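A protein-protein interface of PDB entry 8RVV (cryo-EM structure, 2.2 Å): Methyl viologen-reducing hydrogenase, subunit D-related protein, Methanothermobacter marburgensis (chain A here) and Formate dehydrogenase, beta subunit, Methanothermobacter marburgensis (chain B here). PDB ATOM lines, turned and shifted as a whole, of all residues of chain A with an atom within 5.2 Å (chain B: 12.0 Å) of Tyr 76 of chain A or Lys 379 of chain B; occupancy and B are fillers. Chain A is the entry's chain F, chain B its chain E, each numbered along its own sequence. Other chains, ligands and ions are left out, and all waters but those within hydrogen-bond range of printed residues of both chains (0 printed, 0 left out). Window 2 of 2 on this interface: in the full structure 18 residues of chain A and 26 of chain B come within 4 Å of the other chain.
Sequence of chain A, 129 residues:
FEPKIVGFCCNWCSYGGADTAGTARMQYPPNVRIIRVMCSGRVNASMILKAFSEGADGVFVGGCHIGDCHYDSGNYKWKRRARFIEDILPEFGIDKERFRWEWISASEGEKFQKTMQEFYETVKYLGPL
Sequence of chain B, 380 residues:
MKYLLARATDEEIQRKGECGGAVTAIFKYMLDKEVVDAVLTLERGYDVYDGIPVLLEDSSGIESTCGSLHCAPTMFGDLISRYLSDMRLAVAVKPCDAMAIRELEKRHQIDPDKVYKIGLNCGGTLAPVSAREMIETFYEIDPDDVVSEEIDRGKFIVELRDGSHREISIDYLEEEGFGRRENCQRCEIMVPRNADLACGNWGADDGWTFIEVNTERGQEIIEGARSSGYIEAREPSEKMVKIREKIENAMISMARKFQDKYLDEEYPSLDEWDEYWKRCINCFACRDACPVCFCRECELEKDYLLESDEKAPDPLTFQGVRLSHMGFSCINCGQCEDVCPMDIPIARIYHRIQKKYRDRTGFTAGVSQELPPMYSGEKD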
ATOM      1  N   ILE A  66      -4.886   4.255  16.687  1.00  0.00           N
ATOM      2  CA  ILE A  66      -4.885   2.882  16.205  1.00  0.00           C
ATOM      3  C   ILE A  66      -6.199   2.226  16.600  1.00  0.00           C
ATOM      4  O   ILE A  66      -6.577   2.217  17.777  1.00  0.00           O
ATOM      5  CB  ILE A  66      -3.674   2.126  16.756  1.00  0.00           C
ATOM      6  CG1 ILE A  66      -2.379   2.687  16.156  1.00  0.00           C
ATOM      7  CG2 ILE A  66      -3.801   0.648  16.478  1.00  0.00           C
ATOM      8  CD1 ILE A  66      -2.270   2.561  14.645  1.00  0.00           C
ATOM      9  N   GLY A  67      -6.904   1.681  15.613  1.00  0.00           N
ATOM     10  CA  GLY A  67      -8.243   1.170  15.795  1.00  0.00           C
ATOM     11  C   GLY A  67      -9.343   2.154  15.458  1.00  0.00           C
ATOM     12  O   GLY A  67     -10.518   1.773  15.487  1.00  0.00           O
ATOM     13  N   ASP A  72      -9.897   2.096   8.385  1.00  0.00           N
ATOM     14  CA  ASP A  72      -9.823   0.919   9.241  1.00  0.00           C
ATOM     15  C   ASP A  72      -8.462   0.236   9.323  1.00  0.00           C
ATOM     16  O   ASP A  72      -8.234  -0.544  10.251  1.00  0.00           O
ATOM     17  CB  ASP A  72     -10.877  -0.095   8.763  1.00  0.00           C
ATOM     18  CG  ASP A  72     -10.541  -1.515   9.142  1.00  0.00           C
ATOM     19  OD1 ASP A  72     -10.157  -2.288   8.241  1.00  0.00           O
ATOM     20  OD2 ASP A  72     -10.661  -1.866  10.333  1.00  0.00           O
ATOM     21  N   SER A  73      -7.524   0.537   8.422  1.00  0.00           N
ATOM     22  CA  SER A  73      -6.198  -0.056   8.567  1.00  0.00           C
ATOM     23  C   SER A  73      -5.084   0.852   8.060  1.00  0.00           C
ATOM     24  O   SER A  73      -3.915   0.452   8.057  1.00  0.00           O
ATOM     25  CB  SER A  73      -6.127  -1.408   7.856  1.00  0.00           C
ATOM     26  OG  SER A  73      -6.700  -1.339   6.562  1.00  0.00           O
ATOM     27  N   GLY A  74      -5.408   2.071   7.632  1.00  0.00           N
ATOM     28  CA  GLY A  74      -4.400   2.902   6.993  1.00  0.00           C
ATOM     29  C   GLY A  74      -3.311   3.357   7.947  1.00  0.00           C
ATOM     30  O   GLY A  74      -2.124   3.372   7.593  1.00  0.00           O
ATOM     31  N   ASN A  75      -3.692   3.734   9.167  1.00  0.00           N
ATOM     32  CA  ASN A  75      -2.703   4.244  10.107  1.00  0.00           C
ATOM     33  C   ASN A  75      -1.694   3.176  10.503  1.00  0.00           C
ATOM     34  O   ASN A  75      -0.568   3.510  10.875  1.00  0.00           O
ATOM     35  CB  ASN A  75      -3.385   4.826  11.347  1.00  0.00           C
ATOM     36  CG  ASN A  75      -4.447   3.918  11.924  1.00  0.00           C
ATOM     37  OD1 ASN A  75      -4.712   2.838  11.405  1.00  0.00           O
ATOM     38  ND2 ASN A  75      -5.059   4.356  13.010  1.00  0.00           N
ATOM     39  N   TYR A  76      -2.054   1.894  10.416  1.00  0.00           N
ATOM     40  CA  TYR A  76      -1.071   0.840  10.653  1.00  0.00           C
ATOM     41  C   TYR A  76       0.051   0.902   9.623  1.00  0.00           C
ATOM     42  O   TYR A  76       1.245   0.844   9.964  1.00  0.00           O
ATOM     43  CB  TYR A  76      -1.752  -0.528  10.603  1.00  0.00           C
ATOM     44  CG  TYR A  76      -2.738  -0.779  11.716  1.00  0.00           C
ATOM     45  CD1 TYR A  76      -2.324  -1.288  12.936  1.00  0.00           C
ATOM     46  CD2 TYR A  76      -4.086  -0.520  11.539  1.00  0.00           C
ATOM     47  CE1 TYR A  76      -3.225  -1.523  13.950  1.00  0.00           C
ATOM     48  CE2 TYR A  76      -4.991  -0.751  12.545  1.00  0.00           C
ATOM     49  CZ  TYR A  76      -4.558  -1.256  13.747  1.00  0.00           C
ATOM     50  OH  TYR A  76      -5.463  -1.487  14.754  1.00  0.00           O
ATOM     51  N   LYS A  77      -0.323   1.030   8.352  1.00  0.00           N
ATOM     52  CA  LYS A  77       0.667   1.108   7.289  1.00  0.00           C
ATOM     53  C   LYS A  77       1.514   2.358   7.453  1.00  0.00           C
ATOM     54  O   LYS A  77       2.742   2.322   7.282  1.00  0.00           O
ATOM     55  CB  LYS A  77      -0.008   1.097   5.914  1.00  0.00           C
ATOM     56  CG  LYS A  77      -1.305   0.286   5.791  1.00  0.00           C
ATOM     57  CD  LYS A  77      -1.050  -1.134   5.362  1.00  0.00           C
ATOM     58  CE  LYS A  77      -2.352  -1.857   5.089  1.00  0.00           C
ATOM     59  NZ  LYS A  77      -3.105  -2.117   6.341  1.00  0.00           N
ATOM     60  N   TRP A  78       0.877   3.475   7.814  1.00  0.00           N
ATOM     61  CA  TRP A  78       1.661   4.675   8.073  1.00  0.00           C
ATOM     62  C   TRP A  78       2.642   4.456   9.217  1.00  0.00           C
ATOM     63  O   TRP A  78       3.777   4.932   9.163  1.00  0.00           O
ATOM     64  CB  TRP A  78       0.777   5.868   8.402  1.00  0.00           C
ATOM     65  CG  TRP A  78       1.614   6.904   9.057  1.00  0.00           C
ATOM     66  CD1 TRP A  78       1.477   7.398  10.313  1.00  0.00           C
ATOM     67  CD2 TRP A  78       2.774   7.529   8.501  1.00  0.00           C
ATOM     68  NE1 TRP A  78       2.469   8.310  10.571  1.00  0.00           N
ATOM     69  CE2 TRP A  78       3.279   8.407   9.472  1.00  0.00           C
ATOM     70  CE3 TRP A  78       3.431   7.433   7.271  1.00  0.00           C
ATOM     71  CZ2 TRP A  78       4.406   9.189   9.252  1.00  0.00           C
ATOM     72  CZ3 TRP A  78       4.546   8.208   7.054  1.00  0.00           C
ATOM     73  CH2 TRP A  78       5.023   9.076   8.039  1.00  0.00           C
ATOM     74  N   LYS A  79       2.209   3.785  10.282  1.00  0.00           N
ATOM     75  CA  LYS A  79       3.083   3.584  11.430  1.00  0.00           C
ATOM     76  C   LYS A  79       4.326   2.796  11.036  1.00  0.00           C
ATOM     77  O   LYS A  79       5.451   3.130  11.445  1.00  0.00           O
ATOM     78  CB  LYS A  79       2.301   2.873  12.534  1.00  0.00           C
ATOM     79  CG  LYS A  79       3.136   2.395  13.694  1.00  0.00           C
ATOM     80  CD  LYS A  79       2.344   2.404  14.987  1.00  0.00           C
ATOM     81  CE  LYS A  79       2.651   1.191  15.837  1.00  0.00           C
ATOM     82  NZ  LYS A  79       1.794   0.037  15.473  1.00  0.00           N
ATOM     83  N   ARG A  80       4.141   1.752  10.227  1.00  0.00           N
ATOM     84  CA  ARG A  80       5.291   1.012   9.712  1.00  0.00           C
ATOM     85  C   ARG A  80       6.217   1.927   8.914  1.00  0.00           C
ATOM     86  O   ARG A  80       7.445   1.945   9.123  1.00  0.00           O
ATOM     87  CB  ARG A  80       4.809  -0.151   8.849  1.00  0.00           C
ATOM     88  CG  ARG A  80       3.917  -1.139   9.575  1.00  0.00           C
ATOM     89  CD  ARG A  80       3.463  -2.249   8.652  1.00  0.00           C
ATOM     90  NE  ARG A  80       2.180  -2.815   9.055  1.00  0.00           N
ATOM     91  CZ  ARG A  80       1.212  -3.175   8.221  1.00  0.00           C
ATOM     92  NH1 ARG A  80       1.341  -3.051   6.910  1.00  0.00           N
ATOM     93  NH2 ARG A  80       0.085  -3.678   8.716  1.00  0.00           N
ATOM     94  N   ARG A  81       5.640   2.712   8.000  1.00  0.00           N
ATOM     95  CA  ARG A  81       6.451   3.610   7.187  1.00  0.00           C
ATOM     96  C   ARG A  81       7.221   4.592   8.057  1.00  0.00           C
ATOM     97  O   ARG A  81       8.375   4.918   7.765  1.00  0.00           O
ATOM     98  CB  ARG A  81       5.566   4.363   6.199  1.00  0.00           C
ATOM     99  CG  ARG A  81       5.117   3.540   5.013  1.00  0.00           C
ATOM    100  CD  ARG A  81       4.073   4.271   4.199  1.00  0.00           C
ATOM    101  NE  ARG A  81       3.171   3.361   3.505  1.00  0.00           N
ATOM    102  CZ  ARG A  81       1.944   3.675   3.117  1.00  0.00           C
ATOM    103  NH1 ARG A  81       1.435   4.874   3.341  1.00  0.00           N
ATOM    104  NH2 ARG A  81       1.211   2.767   2.481  1.00  0.00           N
ATOM    105  N   TYR B 357      16.054  -2.626   9.890  1.00  0.00           N
ATOM    106  CA  TYR B 357      14.692  -3.098   9.655  1.00  0.00           C
ATOM    107  C   TYR B 357      14.523  -4.552  10.078  1.00  0.00           C
ATOM    108  O   TYR B 357      13.515  -4.912  10.695  1.00  0.00           O
ATOM    109  CB  TYR B 357      14.328  -2.936   8.184  1.00  0.00           C
ATOM    110  CG  TYR B 357      12.898  -3.304   7.873  1.00  0.00           C
ATOM    111  CD1 TYR B 357      11.876  -2.393   8.064  1.00  0.00           C
ATOM    112  CD2 TYR B 357      12.574  -4.561   7.387  1.00  0.00           C
ATOM    113  CE1 TYR B 357      10.574  -2.719   7.783  1.00  0.00           C
ATOM    114  CE2 TYR B 357      11.272  -4.898   7.104  1.00  0.00           C
ATOM    115  CZ  TYR B 357      10.274  -3.971   7.303  1.00  0.00           C
ATOM    116  OH  TYR B 357       8.970  -4.292   7.022  1.00  0.00           O
ATOM    117  N   ARG B 360      14.374  -4.885  13.812  1.00  0.00           N
ATOM    118  CA  ARG B 360      13.091  -4.447  14.345  1.00  0.00           C
ATOM    119  C   ARG B 360      11.985  -5.465  14.076  1.00  0.00           C
ATOM    120  O   ARG B 360      11.258  -5.860  14.994  1.00  0.00           O
ATOM    121  CB  ARG B 360      12.723  -3.092  13.753  1.00  0.00           C
ATOM    122  CG  ARG B 360      11.618  -2.398  14.490  1.00  0.00           C
ATOM    123  CD  ARG B 360      11.731  -0.915  14.313  1.00  0.00           C
ATOM    124  NE  ARG B 360      11.972  -0.524  12.930  1.00  0.00           N
ATOM    125  CZ  ARG B 360      11.072  -0.602  11.960  1.00  0.00           C
ATOM    126  NH1 ARG B 360       9.855  -1.067  12.181  1.00  0.00           N
ATOM    127  NH2 ARG B 360      11.399  -0.192  10.740  1.00  0.00           N
ATOM    128  N   THR B 361      11.837  -5.904  12.826  1.00  0.00           N
ATOM    129  CA  THR B 361      10.670  -6.671  12.411  1.00  0.00           C
ATOM    130  C   THR B 361      10.946  -8.148  12.169  1.00  0.00           C
ATOM    131  O   THR B 361       9.993  -8.915  12.005  1.00  0.00           O
ATOM    132  CB  THR B 361      10.062  -6.079  11.128  1.00  0.00           C
ATOM    133  OG1 THR B 361      10.796  -6.541   9.991  1.00  0.00           O
ATOM    134  CG2 THR B 361      10.087  -4.565  11.157  1.00  0.00           C
ATOM    135  N   PRO B 372       7.702  -8.037   2.851  1.00  0.00           N
ATOM    136  CA  PRO B 372       8.112  -7.404   4.098  1.00  0.00           C
ATOM    137  C   PRO B 372       6.901  -6.939   4.881  1.00  0.00           C
ATOM    138  O   PRO B 372       5.855  -6.602   4.296  1.00  0.00           O
ATOM    139  CB  PRO B 372       8.971  -6.221   3.633  1.00  0.00           C
ATOM    140  CG  PRO B 372       9.291  -6.479   2.213  1.00  0.00           C
ATOM    141  CD  PRO B 372       8.228  -7.344   1.666  1.00  0.00           C
ATOM    142  N   PRO B 373       6.996  -6.896   6.216  1.00  0.00           N
ATOM    143  CA  PRO B 373       5.854  -6.439   7.024  1.00  0.00           C
ATOM    144  C   PRO B 373       5.319  -5.086   6.586  1.00  0.00           C
ATOM    145  O   PRO B 373       4.187  -4.722   6.915  1.00  0.00           O
ATOM    146  CB  PRO B 373       6.430  -6.375   8.443  1.00  0.00           C
ATOM    147  CG  PRO B 373       7.576  -7.301   8.438  1.00  0.00           C
ATOM    148  CD  PRO B 373       8.132  -7.318   7.052  1.00  0.00           C
ATOM    149  N   MET B 374       6.132  -4.329   5.847  1.00  0.00           N
ATOM    150  CA  MET B 374       5.677  -3.054   5.308  1.00  0.00           C
ATOM    151  C   MET B 374       4.410  -3.218   4.483  1.00  0.00           C
ATOM    152  O   MET B 374       3.565  -2.317   4.458  1.00  0.00           O
ATOM    153  CB  MET B 374       6.782  -2.431   4.455  1.00  0.00           C
ATOM    154  CG  MET B 374       6.545  -0.977   4.076  1.00  0.00           C
ATOM    155  SD  MET B 374       6.534   0.145   5.484  1.00  0.00           S
ATOM    156  CE  MET B 374       8.227   0.018   6.043  1.00  0.00           C
ATOM    157  N   TYR B 375       4.259  -4.354   3.803  1.00  0.00           N
ATOM    158  CA  TYR B 375       3.149  -4.579   2.889  1.00  0.00           C
ATOM    159  C   TYR B 375       2.068  -5.477   3.477  1.00  0.00           C
ATOM    160  O   TYR B 375       1.196  -5.940   2.739  1.00  0.00           O
ATOM    161  CB  TYR B 375       3.669  -5.173   1.577  1.00  0.00           C
ATOM    162  CG  TYR B 375       4.619  -4.257   0.844  1.00  0.00           C
ATOM    163  CD1 TYR B 375       4.318  -2.916   0.669  1.00  0.00           C
ATOM    164  CD2 TYR B 375       5.818  -4.730   0.335  1.00  0.00           C
ATOM    165  CE1 TYR B 375       5.180  -2.073   0.008  1.00  0.00           C
ATOM    166  CE2 TYR B 375       6.686  -3.893  -0.332  1.00  0.00           C
ATOM    167  CZ  TYR B 375       6.361  -2.564  -0.491  1.00  0.00           C
ATOM    168  OH  TYR B 375       7.217  -1.721  -1.155  1.00  0.00           O
ATOM    169  N   SER B 376       2.099  -5.730   4.781  1.00  0.00           N
ATOM    170  CA  SER B 376       1.075  -6.557   5.401  1.00  0.00           C
ATOM    171  C   SER B 376      -0.276  -5.860   5.360  1.00  0.00           C
ATOM    172  O   SER B 376      -0.377  -4.646   5.555  1.00  0.00           O
ATOM    173  CB  SER B 376       1.450  -6.875   6.846  1.00  0.00           C
ATOM    174  OG  SER B 376       0.439  -7.648   7.467  1.00  0.00           O
ATOM    175  N   GLY B 377      -1.323  -6.639   5.097  1.00  0.00           N
ATOM    176  CA  GLY B 377      -2.679  -6.131   5.130  1.00  0.00           C
ATOM    177  C   GLY B 377      -3.374  -6.258   6.463  1.00  0.00           C
ATOM    178  O   GLY B 377      -4.460  -5.703   6.641  1.00  0.00           O
ATOM    179  N   GLU B 378      -2.773  -6.971   7.412  1.00  0.00           N
ATOM    180  CA  GLU B 378      -3.390  -7.183   8.709  1.00  0.00           C
ATOM    181  C   GLU B 378      -3.169  -5.972   9.610  1.00  0.00           C
ATOM    182  O   GLU B 378      -2.373  -5.076   9.318  1.00  0.00           O
ATOM    183  CB  GLU B 378      -2.840  -8.443   9.381  1.00  0.00           C
ATOM    184  CG  GLU B 378      -2.562  -9.624   8.450  1.00  0.00           C
ATOM    185  CD  GLU B 378      -3.724 -10.596   8.375  1.00  0.00           C
ATOM    186  OE1 GLU B 378      -4.846 -10.222   8.774  1.00  0.00           O
ATOM    187  OE2 GLU B 378      -3.513 -11.736   7.911  1.00  0.00           O
ATOM    188  N   LYS B 379      -3.898  -5.951  10.722  1.00  0.00           N
ATOM    189  CA  LYS B 379      -3.773  -4.895  11.717  1.00  0.00           C
ATOM    190  C   LYS B 379      -2.577  -5.094  12.637  1.00  0.00           C
ATOM    191  O   LYS B 379      -2.422  -4.335  13.597  1.00  0.00           O
ATOM    192  CB  LYS B 379      -5.051  -4.808  12.550  1.00  0.00           C
ATOM    193  CG  LYS B 379      -6.198  -4.131  11.837  1.00  0.00           C
ATOM    194  CD  LYS B 379      -7.232  -3.622  12.817  1.00  0.00           C
ATOM    195  CE  LYS B 379      -8.601  -3.517  12.177  1.00  0.00           C
ATOM    196  NZ  LYS B 379      -8.565  -2.874  10.837  1.00  0.00           N
ATOM    197  N   ASP B 380      -1.743  -6.093  12.374  1.00  0.00           N
ATOM    198  CA  ASP B 380      -0.540  -6.317  13.161  1.00  0.00           C
ATOM    199  C   ASP B 380       0.322  -5.060  13.201  1.00  0.00           C
ATOM    200  O   ASP B 380       0.386  -4.310  12.226  1.00  0.00           O
ATOM    201  CB  ASP B 380       0.262  -7.485  12.585  1.00  0.00           C
ATOM    202  CG  ASP B 380       0.875  -7.158  11.235  1.00  0.00           C
ATOM    203  OD1 ASP B 380       0.181  -7.322  10.213  1.00  0.00           O
ATOM    204  OD2 ASP B 380       2.049  -6.734  11.198  1.00  0.00           O
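Lys 379 of chain B touches just these residues of chain A: Asp 72 (2.4 Å) and Tyr 76 (2.9 Å).
No residue of chain B comes within 4 Å of Ile 66 of chain A.
No residue of chain B comes within 4 Å of Gly 67 of chain A.
No residue of chain B comes within 4 Å of Ser 73 of chain A.
No residue of chain B comes within 4 Å of Gly 74 of chain A.
No residue of chain B comes within 4 Å of Asn 75 of chain A.
Printed residues of chain B within 4 Å of Lys 77 of chain A: Ser 376 and Gly 377.
Arg 80 of chain A touches just these residues of chain B: Pro 373, Met 374, Ser 376, Glu 378 and Asp 380.
Printed residues of chain B within 4 Å of Arg 81 of chain A: Met 374 (3.7 Å).
Of the printed residues of chain A, Ser 376 of chain B touches Lys 77 and Arg 80.
Printed residues of chain A within 4 Å of Glu 378 of chain B: Arg 80.
Arg 360 of chain B touches none of the printed residues of chain A.
Tyr 76 of chain A touches Lys 379 of chain B.
Lys 77 of chain A touches Ser 376 of chain B (CE to O, 3.4 Å).
Lys 77 of chain A touches Gly 377 of chain B.
OD1 of Asp 380 of chain B lies within hydrogen-bond range of OG of Ser 376 of chain B.
The backbone carbonyl oxygen of Ser 73 of chain A sits at hydrogen-bond distance from the side-chain amino group of Lys 77 of chain A, 3.2 Å away.
The side-chain hydroxyl of Ser 376 of chain B is in hydrogen-bond range of the backbone NH of Glu 378 of chain B (3.3 Å).
The side-chain hydroxyl of Tyr 357 of chain B lies within hydrogen-bond range of the backbone NH of Met 374 of chain B (3.1 Å).
Of the 12 printed residues of chain B, 7 touch a printed residue of chain A.
Hydrophobic or aromatic side chains of chain B that line the printed part of chain A: Met 374.
Printed residues of chain A that touch a printed residue of chain B: Asp 72, Tyr 76, Lys 77, Arg 80 and Arg 81.
Among the printed residues, 10 pairs touch across the chains.
Among the printed residues, Asp or Glu carboxylates within 4 Å of a Lys or Arg side-chain nitrogen of the other chain: Asp 72 of chain A with Lys 379 of chain B and Arg 80 of chain A with Asp 380 of chain B.
The backbone carbonyl oxygen of Glu 378 of chain B sits at hydrogen-bond distance from the guanidinium group of Arg 80 of chain A (2.9 Å).
The side-chain carboxylate of Asp 72 of chain A lies within salt-bridge range of the side-chain amino group of Lys 379 of chain B (3.1 Å).
The backbone NH of Arg 81 of chain A is in hydrogen-bond range of the side-chain sulfur of Met 374 of chain B (3.7 Å).
The backbone carbonyl oxygen of Met 374 of chain B is in hydrogen-bond range of the guanidinium group of Arg 80 of chain A, 3.4 Å away.
The backbone carbonyl oxygen (O) of Ser 376 of chain B sits at hydrogen-bond distance from the guanidinium group (NH1) of Arg 80 of chain A (2.7 Å).
The backbone carbonyl oxygen (O) of Pro 373 of chain B sits close to the guanidinium group (NH1) of Arg 80 of chain A.
The guanidinium group (NH2) of Arg 80 of chain A is in salt-bridge range of the side-chain carboxylate (OD1) of Asp 380 of chain B (3.9 Å).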
